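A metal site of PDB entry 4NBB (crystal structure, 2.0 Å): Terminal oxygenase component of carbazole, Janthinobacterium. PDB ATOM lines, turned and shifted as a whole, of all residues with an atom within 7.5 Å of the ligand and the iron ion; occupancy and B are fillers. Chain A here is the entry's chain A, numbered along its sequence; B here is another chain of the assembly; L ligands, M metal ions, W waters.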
ATOM      1  N   ALA A 174     -16.467  30.414 -18.029  1.00  0.00           N
ATOM      2  CA  ALA A 174     -15.549  30.557 -19.153  1.00  0.00           C
ATOM      3  C   ALA A 174     -14.416  31.538 -18.820  1.00  0.00           C
ATOM      4  O   ALA A 174     -13.237  31.230 -19.037  1.00  0.00           O
ATOM      5  CB  ALA A 174     -16.309  31.019 -20.391  1.00  0.00           C
ATOM      6  N   ASN A 177     -11.998  30.094 -16.213  1.00  0.00           N
ATOM      7  CA  ASN A 177     -11.149  29.040 -16.751  1.00  0.00           C
ATOM      8  C   ASN A 177     -10.029  29.648 -17.581  1.00  0.00           C
ATOM      9  O   ASN A 177      -8.874  29.279 -17.427  1.00  0.00           O
ATOM     10  CB  ASN A 177     -11.947  28.079 -17.635  1.00  0.00           C
ATOM     11  CG  ASN A 177     -11.063  27.052 -18.319  1.00  0.00           C
ATOM     12  OD1 ASN A 177     -10.567  26.127 -17.686  1.00  0.00           O
ATOM     13  ND2 ASN A 177     -10.839  27.227 -19.611  1.00  0.00           N
ATOM     14  N   GLY A 178     -10.364  30.599 -18.441  1.00  0.00           N
ATOM     15  CA  GLY A 178      -9.363  31.225 -19.295  1.00  0.00           C
ATOM     16  C   GLY A 178      -8.256  31.977 -18.566  1.00  0.00           C
ATOM     17  O   GLY A 178      -7.092  31.948 -18.983  1.00  0.00           O
ATOM     18  N   PHE A 179      -8.614  32.649 -17.483  1.00  0.00           N
ATOM     19  CA  PHE A 179      -7.662  33.438 -16.702  1.00  0.00           C
ATOM     20  C   PHE A 179      -6.965  32.626 -15.589  1.00  0.00           C
ATOM     21  O   PHE A 179      -6.060  33.127 -14.926  1.00  0.00           O
ATOM     22  CB  PHE A 179      -8.386  34.648 -16.114  1.00  0.00           C
ATOM     23  CG  PHE A 179      -7.467  35.681 -15.517  1.00  0.00           C
ATOM     24  CD1 PHE A 179      -6.403  36.195 -16.260  1.00  0.00           C
ATOM     25  CD2 PHE A 179      -7.674  36.164 -14.238  1.00  0.00           C
ATOM     26  CE1 PHE A 179      -5.564  37.174 -15.726  1.00  0.00           C
ATOM     27  CE2 PHE A 179      -6.843  37.143 -13.692  1.00  0.00           C
ATOM     28  CZ  PHE A 179      -5.790  37.651 -14.441  1.00  0.00           C
ATOM     29  N   ASP A 180      -7.404  31.389 -15.407  1.00  0.00           N
ATOM     30  CA  ASP A 180      -6.877  30.474 -14.375  1.00  0.00           C
ATOM     31  C   ASP A 180      -5.436  30.059 -14.674  1.00  0.00           C
ATOM     32  O   ASP A 180      -5.196  29.280 -15.599  1.00  0.00           O
ATOM     33  CB  ASP A 180      -7.779  29.234 -14.343  1.00  0.00           C
ATOM     34  CG  ASP A 180      -7.490  28.318 -13.174  1.00  0.00           C
ATOM     35  OD1 ASP A 180      -6.332  28.254 -12.705  1.00  0.00           O
ATOM     36  OD2 ASP A 180      -8.450  27.639 -12.731  1.00  0.00           O
ATOM     37  N   HIS A 183      -4.868  26.175 -14.745  1.00  0.00           N
ATOM     38  CA  HIS A 183      -5.661  25.326 -15.625  1.00  0.00           C
ATOM     39  C   HIS A 183      -4.814  24.818 -16.802  1.00  0.00           C
ATOM     40  O   HIS A 183      -5.213  23.901 -17.504  1.00  0.00           O
ATOM     41  CB  HIS A 183      -6.905  26.067 -16.146  1.00  0.00           C
ATOM     42  CG  HIS A 183      -6.725  26.742 -17.471  1.00  0.00           C
ATOM     43  ND1 HIS A 183      -6.046  27.931 -17.610  1.00  0.00           N
ATOM     44  CD2 HIS A 183      -7.118  26.381 -18.709  1.00  0.00           C
ATOM     45  CE1 HIS A 183      -6.030  28.268 -18.882  1.00  0.00           C
ATOM     46  NE2 HIS A 183      -6.673  27.347 -19.574  1.00  0.00           N
ATOM     47  N   ILE A 184      -3.652  25.430 -16.985  1.00  0.00           N
ATOM     48  CA  ILE A 184      -2.720  25.060 -18.044  1.00  0.00           C
ATOM     49  C   ILE A 184      -2.463  23.541 -18.052  1.00  0.00           C
ATOM     50  O   ILE A 184      -2.082  22.951 -19.061  1.00  0.00           O
ATOM     51  CB  ILE A 184      -1.381  25.832 -17.856  1.00  0.00           C
ATOM     52  CG1 ILE A 184      -0.553  25.815 -19.133  1.00  0.00           C
ATOM     53  CG2 ILE A 184      -0.598  25.221 -16.711  1.00  0.00           C
ATOM     54  CD1 ILE A 184       0.751  26.615 -19.001  1.00  0.00           C
ATOM     55  N   ILE A 186      -4.579  21.172 -18.070  1.00  0.00           N
ATOM     56  CA  ILE A 186      -5.455  20.486 -19.010  1.00  0.00           C
ATOM     57  C   ILE A 186      -4.964  20.536 -20.455  1.00  0.00           C
ATOM     58  O   ILE A 186      -5.493  19.849 -21.316  1.00  0.00           O
ATOM     59  CB  ILE A 186      -6.906  21.044 -19.016  1.00  0.00           C
ATOM     60  CG1 ILE A 186      -6.936  22.403 -19.723  1.00  0.00           C
ATOM     61  CG2 ILE A 186      -7.445  21.159 -17.585  1.00  0.00           C
ATOM     62  CD1 ILE A 186      -8.354  22.942 -19.924  1.00  0.00           C
ATOM     63  N   HIS A 187      -3.955  21.360 -20.711  1.00  0.00           N
ATOM     64  CA  HIS A 187      -3.423  21.525 -22.064  1.00  0.00           C
ATOM     65  C   HIS A 187      -2.146  20.761 -22.317  1.00  0.00           C
ATOM     66  O   HIS A 187      -1.569  20.865 -23.389  1.00  0.00           O
ATOM     67  CB  HIS A 187      -3.161  23.005 -22.334  1.00  0.00           C
ATOM     68  CG  HIS A 187      -4.397  23.846 -22.418  1.00  0.00           C
ATOM     69  ND1 HIS A 187      -5.386  23.634 -23.356  1.00  0.00           N
ATOM     70  CD2 HIS A 187      -4.805  24.918 -21.687  1.00  0.00           C
ATOM     71  CE1 HIS A 187      -6.348  24.524 -23.201  1.00  0.00           C
ATOM     72  NE2 HIS A 187      -6.018  25.314 -22.194  1.00  0.00           N
ATOM     73  N   LEU A 270     -10.281  37.916 -22.644  1.00  0.00           N
ATOM     74  CA  LEU A 270      -8.925  37.539 -22.292  1.00  0.00           C
ATOM     75  C   LEU A 270      -7.935  37.874 -23.400  1.00  0.00           C
ATOM     76  O   LEU A 270      -8.262  37.767 -24.588  1.00  0.00           O
ATOM     77  CB  LEU A 270      -8.856  36.032 -22.017  1.00  0.00           C
ATOM     78  CG  LEU A 270      -7.531  35.441 -21.488  1.00  0.00           C
ATOM     79  CD1 LEU A 270      -7.445  35.669 -19.989  1.00  0.00           C
ATOM     80  CD2 LEU A 270      -7.466  33.940 -21.795  1.00  0.00           C
ATOM     81  N   VAL A 272      -3.993  36.915 -24.488  1.00  0.00           N
ATOM     82  CA  VAL A 272      -2.829  36.082 -24.241  1.00  0.00           C
ATOM     83  C   VAL A 272      -1.782  36.505 -25.262  1.00  0.00           C
ATOM     84  O   VAL A 272      -1.974  36.351 -26.473  1.00  0.00           O
ATOM     85  CB  VAL A 272      -3.163  34.579 -24.411  1.00  0.00           C
ATOM     86  CG1 VAL A 272      -1.973  33.714 -23.997  1.00  0.00           C
ATOM     87  CG2 VAL A 272      -4.388  34.238 -23.553  1.00  0.00           C
ATOM     88  N   PHE A 275       0.623  34.431 -28.438  1.00  0.00           N
ATOM     89  CA  PHE A 275      -0.024  33.134 -28.537  1.00  0.00           C
ATOM     90  C   PHE A 275      -0.803  33.045 -29.853  1.00  0.00           C
ATOM     91  O   PHE A 275      -1.421  34.018 -30.272  1.00  0.00           O
ATOM     92  CB  PHE A 275      -1.005  32.947 -27.374  1.00  0.00           C
ATOM     93  CG  PHE A 275      -1.369  31.518 -27.111  1.00  0.00           C
ATOM     94  CD1 PHE A 275      -0.543  30.705 -26.326  1.00  0.00           C
ATOM     95  CD2 PHE A 275      -2.513  30.972 -27.676  1.00  0.00           C
ATOM     96  CE1 PHE A 275      -0.865  29.371 -26.125  1.00  0.00           C
ATOM     97  CE2 PHE A 275      -2.841  29.627 -27.470  1.00  0.00           C
ATOM     98  CZ  PHE A 275      -2.024  28.829 -26.699  1.00  0.00           C
ATOM     99  N   GLN A 282      -3.626  36.345 -28.873  1.00  0.00           N
ATOM    100  CA  GLN A 282      -4.999  35.872 -28.877  1.00  0.00           C
ATOM    101  C   GLN A 282      -5.902  36.707 -27.994  1.00  0.00           C
ATOM    102  O   GLN A 282      -5.540  37.045 -26.881  1.00  0.00           O
ATOM    103  CB  GLN A 282      -5.044  34.414 -28.401  1.00  0.00           C
ATOM    104  CG  GLN A 282      -6.410  33.751 -28.513  1.00  0.00           C
ATOM    105  CD  GLN A 282      -6.318  32.237 -28.456  1.00  0.00           C
ATOM    106  OE1 GLN A 282      -5.330  31.661 -28.896  1.00  0.00           O
ATOM    107  NE2 GLN A 282      -7.353  31.594 -27.944  1.00  0.00           N
ATOM    108  N   GLU A 284      -9.918  36.627 -26.739  1.00  0.00           N
ATOM    109  CA  GLU A 284     -11.164  35.869 -26.747  1.00  0.00           C
ATOM    110  C   GLU A 284     -12.180  36.369 -25.747  1.00  0.00           C
ATOM    111  O   GLU A 284     -11.857  36.632 -24.579  1.00  0.00           O
ATOM    112  CB  GLU A 284     -10.887  34.378 -26.521  1.00  0.00           C
ATOM    113  CG  GLU A 284     -10.025  34.060 -25.321  1.00  0.00           C
ATOM    114  CD  GLU A 284      -9.849  32.563 -25.147  1.00  0.00           C
ATOM    115  OE1 GLU A 284      -9.588  31.886 -26.165  1.00  0.00           O
ATOM    116  OE2 GLU A 284      -9.971  32.064 -24.013  1.00  0.00           O
ATOM    117  N   TYR A 286     -16.092  35.905 -23.866  1.00  0.00           N
ATOM    118  CA  TYR A 286     -17.009  34.900 -23.352  1.00  0.00           C
ATOM    119  C   TYR A 286     -18.264  35.752 -23.166  1.00  0.00           C
ATOM    120  O   TYR A 286     -18.499  36.312 -22.091  1.00  0.00           O
ATOM    121  CB  TYR A 286     -16.516  34.352 -22.006  1.00  0.00           C
ATOM    122  CG  TYR A 286     -15.041  34.019 -22.007  1.00  0.00           C
ATOM    123  CD1 TYR A 286     -14.563  32.862 -22.615  1.00  0.00           C
ATOM    124  CD2 TYR A 286     -14.112  34.894 -21.444  1.00  0.00           C
ATOM    125  CE1 TYR A 286     -13.194  32.569 -22.650  1.00  0.00           C
ATOM    126  CE2 TYR A 286     -12.743  34.617 -21.463  1.00  0.00           C
ATOM    127  CZ  TYR A 286     -12.298  33.458 -22.075  1.00  0.00           C
ATOM    128  OH  TYR A 286     -10.952  33.168 -22.074  1.00  0.00           O
ATOM    129  N   TYR A 296     -18.390  31.903 -27.510  1.00  0.00           N
ATOM    130  CA  TYR A 296     -16.951  31.789 -27.298  1.00  0.00           C
ATOM    131  C   TYR A 296     -16.376  32.405 -28.577  1.00  0.00           C
ATOM    132  O   TYR A 296     -16.157  31.724 -29.596  1.00  0.00           O
ATOM    133  CB  TYR A 296     -16.543  30.319 -27.117  1.00  0.00           C
ATOM    134  CG  TYR A 296     -15.045  30.107 -26.937  1.00  0.00           C
ATOM    135  CD1 TYR A 296     -14.251  31.073 -26.313  1.00  0.00           C
ATOM    136  CD2 TYR A 296     -14.423  28.943 -27.390  1.00  0.00           C
ATOM    137  CE1 TYR A 296     -12.876  30.888 -26.160  1.00  0.00           C
ATOM    138  CE2 TYR A 296     -13.050  28.756 -27.247  1.00  0.00           C
ATOM    139  CZ  TYR A 296     -12.283  29.731 -26.631  1.00  0.00           C
ATOM    140  OH  TYR A 296     -10.915  29.582 -26.543  1.00  0.00           O
ATOM    141  N   PHE A 329      -6.053  23.455 -29.383  1.00  0.00           N
ATOM    142  CA  PHE A 329      -5.663  23.834 -28.032  1.00  0.00           C
ATOM    143  C   PHE A 329      -6.871  24.148 -27.154  1.00  0.00           C
ATOM    144  O   PHE A 329      -7.065  23.535 -26.107  1.00  0.00           O
ATOM    145  CB  PHE A 329      -4.726  25.036 -28.090  1.00  0.00           C
ATOM    146  CG  PHE A 329      -4.092  25.392 -26.771  1.00  0.00           C
ATOM    147  CD1 PHE A 329      -2.933  24.749 -26.341  1.00  0.00           C
ATOM    148  CD2 PHE A 329      -4.618  26.406 -25.985  1.00  0.00           C
ATOM    149  CE1 PHE A 329      -2.318  25.106 -25.158  1.00  0.00           C
ATOM    150  CE2 PHE A 329      -4.006  26.787 -24.789  1.00  0.00           C
ATOM    151  CZ  PHE A 329      -2.851  26.139 -24.377  1.00  0.00           C
ATOM    152  N   ASN A 330      -7.695  25.098 -27.598  1.00  0.00           N
ATOM    153  CA  ASN A 330      -8.858  25.530 -26.824  1.00  0.00           C
ATOM    154  C   ASN A 330     -10.049  24.585 -26.705  1.00  0.00           C
ATOM    155  O   ASN A 330     -10.935  24.828 -25.892  1.00  0.00           O
ATOM    156  CB  ASN A 330      -9.335  26.901 -27.323  1.00  0.00           C
ATOM    157  CG  ASN A 330      -8.288  27.995 -27.109  1.00  0.00           C
ATOM    158  OD1 ASN A 330      -7.937  28.717 -28.033  1.00  0.00           O
ATOM    159  ND2 ASN A 330      -7.789  28.106 -25.882  1.00  0.00           N
ATOM    160  N   ASP A 332     -10.140  21.826 -25.331  1.00  0.00           N
ATOM    161  CA  ASP A 332     -10.138  21.278 -23.970  1.00  0.00           C
ATOM    162  C   ASP A 332     -10.716  22.277 -22.973  1.00  0.00           C
ATOM    163  O   ASP A 332     -11.239  21.887 -21.933  1.00  0.00           O
ATOM    164  CB  ASP A 332      -8.728  20.864 -23.541  1.00  0.00           C
ATOM    165  CG  ASP A 332      -8.272  19.579 -24.188  1.00  0.00           C
ATOM    166  OD1 ASP A 332      -9.104  18.637 -24.273  1.00  0.00           O
ATOM    167  OD2 ASP A 332      -7.102  19.486 -24.605  1.00  0.00           O
ATOM    168  N   ASP A 333     -10.619  23.571 -23.275  1.00  0.00           N
ATOM    169  CA  ASP A 333     -11.189  24.575 -22.390  1.00  0.00           C
ATOM    170  C   ASP A 333     -12.705  24.463 -22.412  1.00  0.00           C
ATOM    171  O   ASP A 333     -13.368  24.664 -21.394  1.00  0.00           O
ATOM    172  CB  ASP A 333     -10.799  25.986 -22.836  1.00  0.00           C
ATOM    173  CG  ASP A 333      -9.333  26.281 -22.640  1.00  0.00           C
ATOM    174  OD1 ASP A 333      -8.847  26.235 -21.487  1.00  0.00           O
ATOM    175  OD2 ASP A 333      -8.653  26.557 -23.652  1.00  0.00           O
ATOM    176  N   ILE A 334     -13.252  24.112 -23.578  1.00  0.00           N
ATOM    177  CA  ILE A 334     -14.702  23.994 -23.709  1.00  0.00           C
ATOM    178  C   ILE A 334     -15.301  22.962 -22.767  1.00  0.00           C
ATOM    179  O   ILE A 334     -16.212  23.280 -22.007  1.00  0.00           O
ATOM    180  CB  ILE A 334     -15.122  23.652 -25.163  1.00  0.00           C
ATOM    181  CG1 ILE A 334     -14.770  24.821 -26.090  1.00  0.00           C
ATOM    182  CG2 ILE A 334     -16.619  23.354 -25.212  1.00  0.00           C
ATOM    183  CD1 ILE A 334     -14.998  24.556 -27.589  1.00  0.00           C
ATOM    184  N   ALA A 336     -13.908  21.706 -20.182  1.00  0.00           N
ATOM    185  CA  ALA A 336     -13.505  22.019 -18.811  1.00  0.00           C
ATOM    186  C   ALA A 336     -14.545  22.986 -18.236  1.00  0.00           C
ATOM    187  O   ALA A 336     -14.940  22.871 -17.068  1.00  0.00           O
ATOM    188  CB  ALA A 336     -12.127  22.649 -18.798  1.00  0.00           C
ATOM    189  N   ARG A 337     -14.996  23.941 -19.050  1.00  0.00           N
ATOM    190  CA  ARG A 337     -16.004  24.914 -18.613  1.00  0.00           C
ATOM    191  C   ARG A 337     -17.293  24.195 -18.302  1.00  0.00           C
ATOM    192  O   ARG A 337     -17.942  24.452 -17.295  1.00  0.00           O
ATOM    193  CB  ARG A 337     -16.311  25.942 -19.708  1.00  0.00           C
ATOM    194  CG  ARG A 337     -15.182  26.828 -20.086  1.00  0.00           C
ATOM    195  CD  ARG A 337     -15.564  27.676 -21.266  1.00  0.00           C
ATOM    196  NE  ARG A 337     -14.370  28.103 -21.974  1.00  0.00           N
ATOM    197  CZ  ARG A 337     -14.355  28.629 -23.192  1.00  0.00           C
ATOM    198  NH1 ARG A 337     -15.495  28.811 -23.856  1.00  0.00           N
ATOM    199  NH2 ARG A 337     -13.199  28.950 -23.759  1.00  0.00           N
ATOM    200  N   TYR B  92      -8.307  18.625 -13.876  1.00  0.00           N
ATOM    201  CA  TYR B  92      -8.319  20.081 -14.006  1.00  0.00           C
ATOM    202  C   TYR B  92      -7.054  20.794 -13.502  1.00  0.00           C
ATOM    203  O   TYR B  92      -6.292  21.331 -14.297  1.00  0.00           O
ATOM    204  CB  TYR B  92      -9.560  20.654 -13.296  1.00  0.00           C
ATOM    205  CG  TYR B  92     -10.141  21.912 -13.918  1.00  0.00           C
ATOM    206  CD1 TYR B  92      -9.452  22.608 -14.925  1.00  0.00           C
ATOM    207  CD2 TYR B  92     -11.369  22.417 -13.479  1.00  0.00           C
ATOM    208  CE1 TYR B  92      -9.981  23.796 -15.469  1.00  0.00           C
ATOM    209  CE2 TYR B  92     -11.901  23.584 -14.015  1.00  0.00           C
ATOM    210  CZ  TYR B  92     -11.214  24.275 -14.998  1.00  0.00           C
ATOM    211  OH  TYR B  92     -11.759  25.431 -15.518  1.00  0.00           O
HETATM  212  O1  LIG L   1      -6.013  28.704 -22.257  1.00  0.00           O
HETATM  213  O2  LIG L   1      -7.452  28.688 -22.263  1.00  0.00           O
HETATM  214 FE    FE M   1      -7.083  26.973 -21.526  1.00  0.00          FE
HETATM  215  O   HOH W   1     -10.131  29.414 -22.953  1.00  0.00           O
HETATM  216  O   HOH W   2      -2.899  30.161 -22.803  1.00  0.00           O
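The side-chain amide nitrogen of Asn 330 lies within hydrogen-bond range of the side-chain carboxylate of Asp 333. ND1 of His 187 lies close to O of Phe 329 (3.2 Å). ND1 of His 183 is in hydrogen-bond range of O of Asn 177, at 3.1 Å. The side-chain carboxylate of Asp 333 lies close to the side-chain amide nitrogen of Asn 177 (2.9 Å). The side-chain amide nitrogen (NE2) of Gln 282 is in hydrogen-bond range of the side-chain amide oxygen (OD1) of Asn 330. A ring nitrogen (ND1) of His 183 is in hydrogen-bond range of the backbone carbonyl oxygen (O) of Asp 180 (2.6 Å). The side-chain amide oxygen (OD1) of Asn 330 lies close to the side-chain hydroxyl (OH) of Tyr 296, at 3.4 Å.
Water W1 lies within hydrogen-bond range of the side-chain carboxylate of Glu 284, the guanidinium group of Arg 337 and the side-chain carboxylate of Asp 333.
Merely in contact with the ligand: Asn 330 (3.7 Å) and Phe 329 (3.8 Å). Hydrophobic or aromatic side chains that line the ligand: His 183 and Phe 329. Of the 24 residues printed, 5 come within 4 Å of the ligand. The nearest printed residue that does not touch the ligand is Gly 178 (4.3 Å).
The iron ion is bound by O2 of the ligand (1.9 Å), OD1 of Asp 333 (1.9 Å), NE2 of His 183 (2.0 Å) and NE2 of His 187 (2.1 Å). The iron ion has four donor atoms within binding distance. Slightly farther from the iron ion lies the side-chain carboxylate (OD2) of Asp 333 (2.7 Å).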
